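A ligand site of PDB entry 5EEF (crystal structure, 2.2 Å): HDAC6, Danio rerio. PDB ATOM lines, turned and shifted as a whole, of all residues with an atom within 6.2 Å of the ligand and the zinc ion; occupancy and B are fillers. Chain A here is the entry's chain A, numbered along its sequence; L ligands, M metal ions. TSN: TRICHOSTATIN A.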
ATOM      1  N   HIS A  29     -14.075 -22.602 -33.484  1.00  0.00           N
ATOM      2  CA  HIS A  29     -15.112 -23.525 -33.054  1.00  0.00           C
ATOM      3  C   HIS A  29     -15.411 -23.442 -31.564  1.00  0.00           C
ATOM      4  O   HIS A  29     -14.491 -23.473 -30.748  1.00  0.00           O
ATOM      5  CB  HIS A  29     -14.733 -24.952 -33.433  1.00  0.00           C
ATOM      6  CG  HIS A  29     -15.909 -25.852 -33.645  1.00  0.00           C
ATOM      7  ND1 HIS A  29     -16.544 -26.502 -32.612  1.00  0.00           N
ATOM      8  CD2 HIS A  29     -16.581 -26.184 -34.771  1.00  0.00           C
ATOM      9  CE1 HIS A  29     -17.544 -27.210 -33.091  1.00  0.00           C
ATOM     10  NE2 HIS A  29     -17.589 -27.031 -34.400  1.00  0.00           N
ATOM     11  N   PRO A  30     -16.702 -23.335 -31.216  1.00  0.00           N
ATOM     12  CA  PRO A  30     -17.169 -23.229 -29.826  1.00  0.00           C
ATOM     13  C   PRO A  30     -16.878 -24.459 -28.974  1.00  0.00           C
ATOM     14  O   PRO A  30     -16.502 -24.303 -27.808  1.00  0.00           O
ATOM     15  CB  PRO A  30     -18.680 -23.024 -29.992  1.00  0.00           C
ATOM     16  CG  PRO A  30     -19.000 -23.559 -31.342  1.00  0.00           C
ATOM     17  CD  PRO A  30     -17.811 -23.222 -32.182  1.00  0.00           C
ATOM     18  N   ASP A  96     -25.583 -33.564 -38.692  1.00  0.00           N
ATOM     19  CA  ASP A  96     -25.955 -32.200 -38.327  1.00  0.00           C
ATOM     20  C   ASP A  96     -24.999 -31.650 -37.267  1.00  0.00           C
ATOM     21  O   ASP A  96     -24.895 -32.194 -36.172  1.00  0.00           O
ATOM     22  CB  ASP A  96     -27.395 -32.159 -37.813  1.00  0.00           C
ATOM     23  CG  ASP A  96     -27.950 -30.746 -37.714  1.00  0.00           C
ATOM     24  OD1 ASP A  96     -27.154 -29.780 -37.669  1.00  0.00           O
ATOM     25  OD2 ASP A  96     -29.186 -30.594 -37.686  1.00  0.00           O
ATOM     26  N   SER A  97     -24.305 -30.574 -37.624  1.00  0.00           N
ATOM     27  CA  SER A  97     -23.412 -29.851 -36.711  1.00  0.00           C
ATOM     28  C   SER A  97     -22.419 -30.772 -36.005  1.00  0.00           C
ATOM     29  O   SER A  97     -22.487 -30.955 -34.786  1.00  0.00           O
ATOM     30  CB  SER A  97     -24.232 -29.082 -35.671  1.00  0.00           C
ATOM     31  OG  SER A  97     -25.142 -28.199 -36.303  1.00  0.00           O
ATOM     32  N   VAL A  98     -21.500 -31.340 -36.784  1.00  0.00           N
ATOM     33  CA  VAL A  98     -20.537 -32.309 -36.278  1.00  0.00           C
ATOM     34  C   VAL A  98     -19.203 -32.211 -37.014  1.00  0.00           C
ATOM     35  O   VAL A  98     -19.163 -32.219 -38.246  1.00  0.00           O
ATOM     36  CB  VAL A  98     -21.079 -33.761 -36.406  1.00  0.00           C
ATOM     37  CG1 VAL A  98     -19.935 -34.771 -36.468  1.00  0.00           C
ATOM     38  CG2 VAL A  98     -22.028 -34.088 -35.271  1.00  0.00           C
ATOM     39  N   PRO A 137     -19.420 -34.033 -25.561  1.00  0.00           N
ATOM     40  CA  PRO A 137     -20.741 -34.214 -24.950  1.00  0.00           C
ATOM     41  C   PRO A 137     -21.486 -35.386 -25.578  1.00  0.00           C
ATOM     42  O   PRO A 137     -20.985 -36.004 -26.517  1.00  0.00           O
ATOM     43  CB  PRO A 137     -21.448 -32.888 -25.246  1.00  0.00           C
ATOM     44  CG  PRO A 137     -20.782 -32.381 -26.476  1.00  0.00           C
ATOM     45  CD  PRO A 137     -19.346 -32.768 -26.323  1.00  0.00           C
ATOM     46  N   HIS A 139     -25.544 -35.859 -25.236  1.00  0.00           N
ATOM     47  CA  HIS A 139     -27.006 -35.904 -25.223  1.00  0.00           C
ATOM     48  C   HIS A 139     -27.671 -35.720 -26.588  1.00  0.00           C
ATOM     49  O   HIS A 139     -28.878 -35.871 -26.709  1.00  0.00           O
ATOM     50  CB  HIS A 139     -27.576 -34.878 -24.225  1.00  0.00           C
ATOM     51  CG  HIS A 139     -27.473 -33.458 -24.678  1.00  0.00           C
ATOM     52  ND1 HIS A 139     -28.506 -32.552 -24.506  1.00  0.00           N
ATOM     53  CD2 HIS A 139     -26.469 -32.760 -25.259  1.00  0.00           C
ATOM     54  CE1 HIS A 139     -28.145 -31.373 -24.978  1.00  0.00           C
ATOM     55  NE2 HIS A 139     -26.910 -31.476 -25.439  1.00  0.00           N
ATOM     56  N   HIS A 140     -26.891 -35.416 -27.625  1.00  0.00           N
ATOM     57  CA  HIS A 140     -27.450 -35.325 -28.980  1.00  0.00           C
ATOM     58  C   HIS A 140     -27.211 -36.585 -29.797  1.00  0.00           C
ATOM     59  O   HIS A 140     -27.856 -36.786 -30.825  1.00  0.00           O
ATOM     60  CB  HIS A 140     -26.885 -34.119 -29.721  1.00  0.00           C
ATOM     61  CG  HIS A 140     -27.326 -32.800 -29.165  1.00  0.00           C
ATOM     62  ND1 HIS A 140     -28.656 -32.454 -29.073  1.00  0.00           N
ATOM     63  CD2 HIS A 140     -26.620 -31.761 -28.671  1.00  0.00           C
ATOM     64  CE1 HIS A 140     -28.745 -31.247 -28.537  1.00  0.00           C
ATOM     65  NE2 HIS A 140     -27.525 -30.810 -28.286  1.00  0.00           N
ATOM     66  N   GLY A 148     -24.842 -32.852 -33.211  1.00  0.00           N
ATOM     67  CA  GLY A 148     -24.562 -31.793 -32.272  1.00  0.00           C
ATOM     68  C   GLY A 148     -23.306 -31.989 -31.448  1.00  0.00           C
ATOM     69  O   GLY A 148     -23.360 -31.925 -30.223  1.00  0.00           O
ATOM     70  N   PHE A 149     -22.196 -32.259 -32.130  1.00  0.00           N
ATOM     71  CA  PHE A 149     -20.869 -32.426 -31.532  1.00  0.00           C
ATOM     72  C   PHE A 149     -20.779 -33.660 -30.619  1.00  0.00           C
ATOM     73  O   PHE A 149     -19.850 -33.765 -29.808  1.00  0.00           O
ATOM     74  CB  PHE A 149     -20.474 -31.166 -30.739  1.00  0.00           C
ATOM     75  CG  PHE A 149     -20.740 -29.885 -31.469  1.00  0.00           C
ATOM     76  CD1 PHE A 149     -20.430 -29.750 -32.814  1.00  0.00           C
ATOM     77  CD2 PHE A 149     -21.304 -28.806 -30.805  1.00  0.00           C
ATOM     78  CE1 PHE A 149     -20.680 -28.572 -33.483  1.00  0.00           C
ATOM     79  CE2 PHE A 149     -21.553 -27.628 -31.474  1.00  0.00           C
ATOM     80  CZ  PHE A 149     -21.243 -27.504 -32.810  1.00  0.00           C
ATOM     81  N   CYS A 150     -21.730 -34.576 -30.768  1.00  0.00           N
ATOM     82  CA  CYS A 150     -21.762 -35.798 -29.969  1.00  0.00           C
ATOM     83  C   CYS A 150     -21.550 -37.035 -30.830  1.00  0.00           C
ATOM     84  O   CYS A 150     -22.191 -37.178 -31.865  1.00  0.00           O
ATOM     85  CB  CYS A 150     -23.091 -35.932 -29.222  1.00  0.00           C
ATOM     86  SG  CYS A 150     -23.607 -34.492 -28.287  1.00  0.00           S
ATOM     87  N   ASP A 177     -29.347 -28.499 -20.065  1.00  0.00           N
ATOM     88  CA  ASP A 177     -28.664 -27.869 -21.181  1.00  0.00           C
ATOM     89  C   ASP A 177     -29.698 -27.050 -21.967  1.00  0.00           C
ATOM     90  O   ASP A 177     -30.869 -27.420 -22.021  1.00  0.00           O
ATOM     91  CB  ASP A 177     -28.012 -28.918 -22.085  1.00  0.00           C
ATOM     92  CG  ASP A 177     -27.098 -28.312 -23.138  1.00  0.00           C
ATOM     93  OD1 ASP A 177     -27.614 -27.655 -24.070  1.00  0.00           O
ATOM     94  OD2 ASP A 177     -25.874 -28.518 -23.046  1.00  0.00           O
ATOM     95  N   VAL A 178     -29.260 -25.948 -22.559  1.00  0.00           N
ATOM     96  CA  VAL A 178     -30.172 -25.062 -23.269  1.00  0.00           C
ATOM     97  C   VAL A 178     -30.679 -25.712 -24.567  1.00  0.00           C
ATOM     98  O   VAL A 178     -31.695 -25.291 -25.129  1.00  0.00           O
ATOM     99  CB  VAL A 178     -29.515 -23.700 -23.582  1.00  0.00           C
ATOM    100  CG1 VAL A 178     -28.661 -23.789 -24.837  1.00  0.00           C
ATOM    101  CG2 VAL A 178     -30.559 -22.603 -23.710  1.00  0.00           C
ATOM    102  N   HIS A 179     -29.966 -26.727 -25.035  1.00  0.00           N
ATOM    103  CA  HIS A 179     -30.358 -27.438 -26.248  1.00  0.00           C
ATOM    104  C   HIS A 179     -31.118 -28.716 -25.909  1.00  0.00           C
ATOM    105  O   HIS A 179     -30.815 -29.386 -24.916  1.00  0.00           O
ATOM    106  CB  HIS A 179     -29.139 -27.776 -27.102  1.00  0.00           C
ATOM    107  CG  HIS A 179     -28.421 -26.572 -27.639  1.00  0.00           C
ATOM    108  ND1 HIS A 179     -27.361 -25.981 -26.983  1.00  0.00           N
ATOM    109  CD2 HIS A 179     -28.620 -25.846 -28.768  1.00  0.00           C
ATOM    110  CE1 HIS A 179     -26.940 -24.949 -27.688  1.00  0.00           C
ATOM    111  NE2 HIS A 179     -27.679 -24.845 -28.764  1.00  0.00           N
ATOM    112  N   TRP A 208     -32.046 -24.261 -32.771  1.00  0.00           N
ATOM    113  CA  TRP A 208     -31.457 -25.576 -33.031  1.00  0.00           C
ATOM    114  C   TRP A 208     -31.787 -26.533 -31.888  1.00  0.00           C
ATOM    115  O   TRP A 208     -31.721 -26.144 -30.717  1.00  0.00           O
ATOM    116  CB  TRP A 208     -29.945 -25.460 -33.209  1.00  0.00           C
ATOM    117  CG  TRP A 208     -29.288 -26.722 -33.697  1.00  0.00           C
ATOM    118  CD1 TRP A 208     -29.022 -27.047 -34.994  1.00  0.00           C
ATOM    119  CD2 TRP A 208     -28.835 -27.821 -32.905  1.00  0.00           C
ATOM    120  NE1 TRP A 208     -28.431 -28.285 -35.056  1.00  0.00           N
ATOM    121  CE2 TRP A 208     -28.304 -28.788 -33.781  1.00  0.00           C
ATOM    122  CE3 TRP A 208     -28.840 -28.095 -31.534  1.00  0.00           C
ATOM    123  CZ2 TRP A 208     -27.777 -29.993 -33.334  1.00  0.00           C
ATOM    124  CZ3 TRP A 208     -28.308 -29.295 -31.094  1.00  0.00           C
ATOM    125  CH2 TRP A 208     -27.787 -30.232 -31.988  1.00  0.00           C
ATOM    126  N   GLY A 268     -25.306 -29.298 -19.154  1.00  0.00           N
ATOM    127  CA  GLY A 268     -24.742 -28.286 -20.021  1.00  0.00           C
ATOM    128  C   GLY A 268     -24.934 -26.965 -19.312  1.00  0.00           C
ATOM    129  O   GLY A 268     -25.843 -26.823 -18.497  1.00  0.00           O
ATOM    130  N   ASP A 270     -24.853 -23.810 -21.094  1.00  0.00           N
ATOM    131  CA  ASP A 270     -25.031 -22.763 -22.084  1.00  0.00           C
ATOM    132  C   ASP A 270     -26.280 -21.924 -21.801  1.00  0.00           C
ATOM    133  O   ASP A 270     -26.583 -20.979 -22.534  1.00  0.00           O
ATOM    134  CB  ASP A 270     -25.100 -23.358 -23.494  1.00  0.00           C
ATOM    135  CG  ASP A 270     -25.658 -24.758 -23.513  1.00  0.00           C
ATOM    136  OD1 ASP A 270     -26.359 -25.146 -22.546  1.00  0.00           O
ATOM    137  OD2 ASP A 270     -25.400 -25.484 -24.500  1.00  0.00           O
ATOM    138  N   LYS A 277     -24.408 -18.795 -27.109  1.00  0.00           N
ATOM    139  CA  LYS A 277     -25.279 -19.699 -27.852  1.00  0.00           C
ATOM    140  C   LYS A 277     -26.666 -19.856 -27.208  1.00  0.00           C
ATOM    141  O   LYS A 277     -27.675 -19.965 -27.907  1.00  0.00           O
ATOM    142  CB  LYS A 277     -24.614 -21.066 -27.971  1.00  0.00           C
ATOM    143  CG  LYS A 277     -23.144 -20.998 -28.371  1.00  0.00           C
ATOM    144  CD  LYS A 277     -22.917 -21.576 -29.759  1.00  0.00           C
ATOM    145  CE  LYS A 277     -21.759 -20.882 -30.448  1.00  0.00           C
ATOM    146  NZ  LYS A 277     -21.528 -21.440 -31.810  1.00  0.00           N
ATOM    147  N   GLU A 307     -22.175 -31.266 -20.662  1.00  0.00           N
ATOM    148  CA  GLU A 307     -22.691 -31.244 -22.024  1.00  0.00           C
ATOM    149  C   GLU A 307     -22.239 -29.962 -22.723  1.00  0.00           C
ATOM    150  O   GLU A 307     -21.062 -29.818 -23.056  1.00  0.00           O
ATOM    151  CB  GLU A 307     -24.213 -31.363 -22.038  1.00  0.00           C
ATOM    152  CG  GLU A 307     -24.752 -32.687 -21.497  1.00  0.00           C
ATOM    153  CD  GLU A 307     -24.534 -33.857 -22.438  1.00  0.00           C
ATOM    154  OE1 GLU A 307     -24.802 -35.010 -22.021  1.00  0.00           O
ATOM    155  OE2 GLU A 307     -24.101 -33.641 -23.581  1.00  0.00           O
ATOM    156  N   GLY A 308     -23.159 -29.030 -22.919  1.00  0.00           N
ATOM    157  CA  GLY A 308     -22.864 -27.784 -23.597  1.00  0.00           C
ATOM    158  C   GLY A 308     -22.356 -26.692 -22.671  1.00  0.00           C
ATOM    159  O   GLY A 308     -22.140 -26.915 -21.481  1.00  0.00           O
ATOM    160  N   GLY A 309     -22.196 -25.501 -23.206  1.00  0.00           N
ATOM    161  CA  GLY A 309     -21.607 -24.373 -22.521  1.00  0.00           C
ATOM    162  C   GLY A 309     -20.353 -23.920 -23.219  1.00  0.00           C
ATOM    163  O   GLY A 309     -19.425 -24.633 -23.362  1.00  0.00           O
ATOM    164  N   TYR A 310     -20.428 -22.694 -23.682  1.00  0.00           N
ATOM    165  CA  TYR A 310     -19.530 -22.120 -24.632  1.00  0.00           C
ATOM    166  C   TYR A 310     -18.898 -20.804 -24.240  1.00  0.00           C
ATOM    167  O   TYR A 310     -18.139 -20.269 -24.976  1.00  0.00           O
ATOM    168  CB  TYR A 310     -20.266 -21.994 -25.918  1.00  0.00           C
ATOM    169  CG  TYR A 310     -20.654 -23.326 -26.403  1.00  0.00           C
ATOM    170  CD1 TYR A 310     -19.722 -24.157 -26.931  1.00  0.00           C
ATOM    171  CD2 TYR A 310     -21.943 -23.774 -26.275  1.00  0.00           C
ATOM    172  CE1 TYR A 310     -20.043 -25.403 -27.328  1.00  0.00           C
ATOM    173  CE2 TYR A 310     -22.288 -25.016 -26.686  1.00  0.00           C
ATOM    174  CZ  TYR A 310     -21.325 -25.819 -27.218  1.00  0.00           C
ATOM    175  OH  TYR A 310     -21.608 -27.045 -27.632  1.00  0.00           O
HETATM  176  O1  TSN L   1     -25.857 -28.903 -25.714  1.00  0.00           O
HETATM  177  O2  TSN L   1     -24.411 -27.213 -27.045  1.00  0.00           O
HETATM  178  O3  TSN L   1     -23.533 -23.110 -32.916  1.00  0.00           O
HETATM  179  N1  TSN L   1     -25.856 -28.866 -27.079  1.00  0.00           N
HETATM  180  N2  TSN L   1     -20.068 -25.316 -37.734  1.00  0.00           N
HETATM  181  C1  TSN L   1     -22.672 -24.432 -34.632  1.00  0.00           C
HETATM  182  C2  TSN L   1     -21.511 -23.719 -34.761  1.00  0.00           C
HETATM  183  C3  TSN L   1     -20.637 -23.998 -35.788  1.00  0.00           C
HETATM  184  C4  TSN L   1     -20.940 -25.004 -36.676  1.00  0.00           C
HETATM  185  C5  TSN L   1     -22.097 -25.697 -36.521  1.00  0.00           C
HETATM  186  C6  TSN L   1     -22.964 -25.427 -35.507  1.00  0.00           C
HETATM  187  C7  TSN L   1     -23.597 -24.137 -33.514  1.00  0.00           C
HETATM  188  C8  TSN L   1     -24.604 -25.179 -33.177  1.00  0.00           C
HETATM  189  C9  TSN L   1     -24.493 -25.569 -31.737  1.00  0.00           C
HETATM  190  C10 TSN L   1     -24.620 -26.803 -31.256  1.00  0.00           C
HETATM  191  C11 TSN L   1     -24.500 -26.938 -29.796  1.00  0.00           C
HETATM  192  C12 TSN L   1     -25.183 -27.847 -29.124  1.00  0.00           C
HETATM  193  C13 TSN L   1     -25.101 -27.964 -27.680  1.00  0.00           C
HETATM  194  C14 TSN L   1     -25.985 -24.636 -33.513  1.00  0.00           C
HETATM  195  C15 TSN L   1     -24.868 -27.964 -32.148  1.00  0.00           C
HETATM  196  C17 TSN L   1     -18.948 -24.466 -38.029  1.00  0.00           C
HETATM  197  C16 TSN L   1     -20.272 -26.484 -38.562  1.00  0.00           C
HETATM  198 ZN    ZN M   1     -26.234 -27.058 -25.563  1.00  0.00          ZN
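Residues that only touch the zinc ion: Gly 308. The nearest printed residue that does not touch the zinc ion is Val 178 (4.1 Å).
Residues that only touch the ligand: Ser 97 (3.6 Å), Gly 148 (3.8 Å), Phe 149 (3.2 Å), Trp 208 (3.7 Å) and Gly 308 (3.8 Å). Hydrophobic or aromatic side chains within 4 Å of the ligand: His 139, His 140, Phe 149, His 179, Trp 208 and Tyr 310. Along chain A the residues within 4 Å of the ligand span positions 97 to 310. The nearest printed residue that does not touch the ligand is Pro 30 (4.2 Å).
The side-chain sulfur of Cys 150 is in hydrogen-bond range of the backbone carbonyl oxygen of Gly 148 (3.2 Å). The side-chain carboxylate (OD2) of Asp 177 lies within hydrogen-bond range of the backbone NH (N) of Gly 308. A ring nitrogen (NE2) of His 139 lies within hydrogen-bond range of a ring nitrogen (NE2) of His 140 (3.0 Å). O of Ser 97 sits close to N of Gly 148 (3.4 Å). O of Ser 97 is in hydrogen-bond range of N of Phe 149 (3.0 Å). The side-chain carboxylate (OD2) of Asp 270 lies close to the backbone NH (N) of Gly 309 (3.5 Å). The backbone NH (N) of His 140 is in hydrogen-bond range of the side-chain sulfur (SG) of Cys 150, 3.5 Å away. The backbone NH of Val 178 lies within hydrogen-bond range of the side-chain carboxylate of Asp 270 (3.0 Å).
O3 of the ligand lies within hydrogen-bond range of NZ of Lys 277. The side-chain hydroxyl (OH) of Tyr 310 lies close to an oxygen (O2) of the ligand. N1 of the ligand lies close to NE2 of His 140, at 2.8 Å. A ring nitrogen (NE2) of His 139 sits close to an oxygen (O1) of the ligand.
The zinc ion is bound by O1 of the ligand (1.9 Å). The side-chain carboxylate (OD2) of Asp 270 binds the zinc ion (2.1 Å). ND1 of His 179 binds the zinc ion, at 2.1 Å. The side-chain carboxylate (OD1) of Asp 177 binds the zinc ion (2.1 Å). The zinc ion is bound by O2 of the ligand (2.4 Å). The zinc ion has five donor atoms within binding distance.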
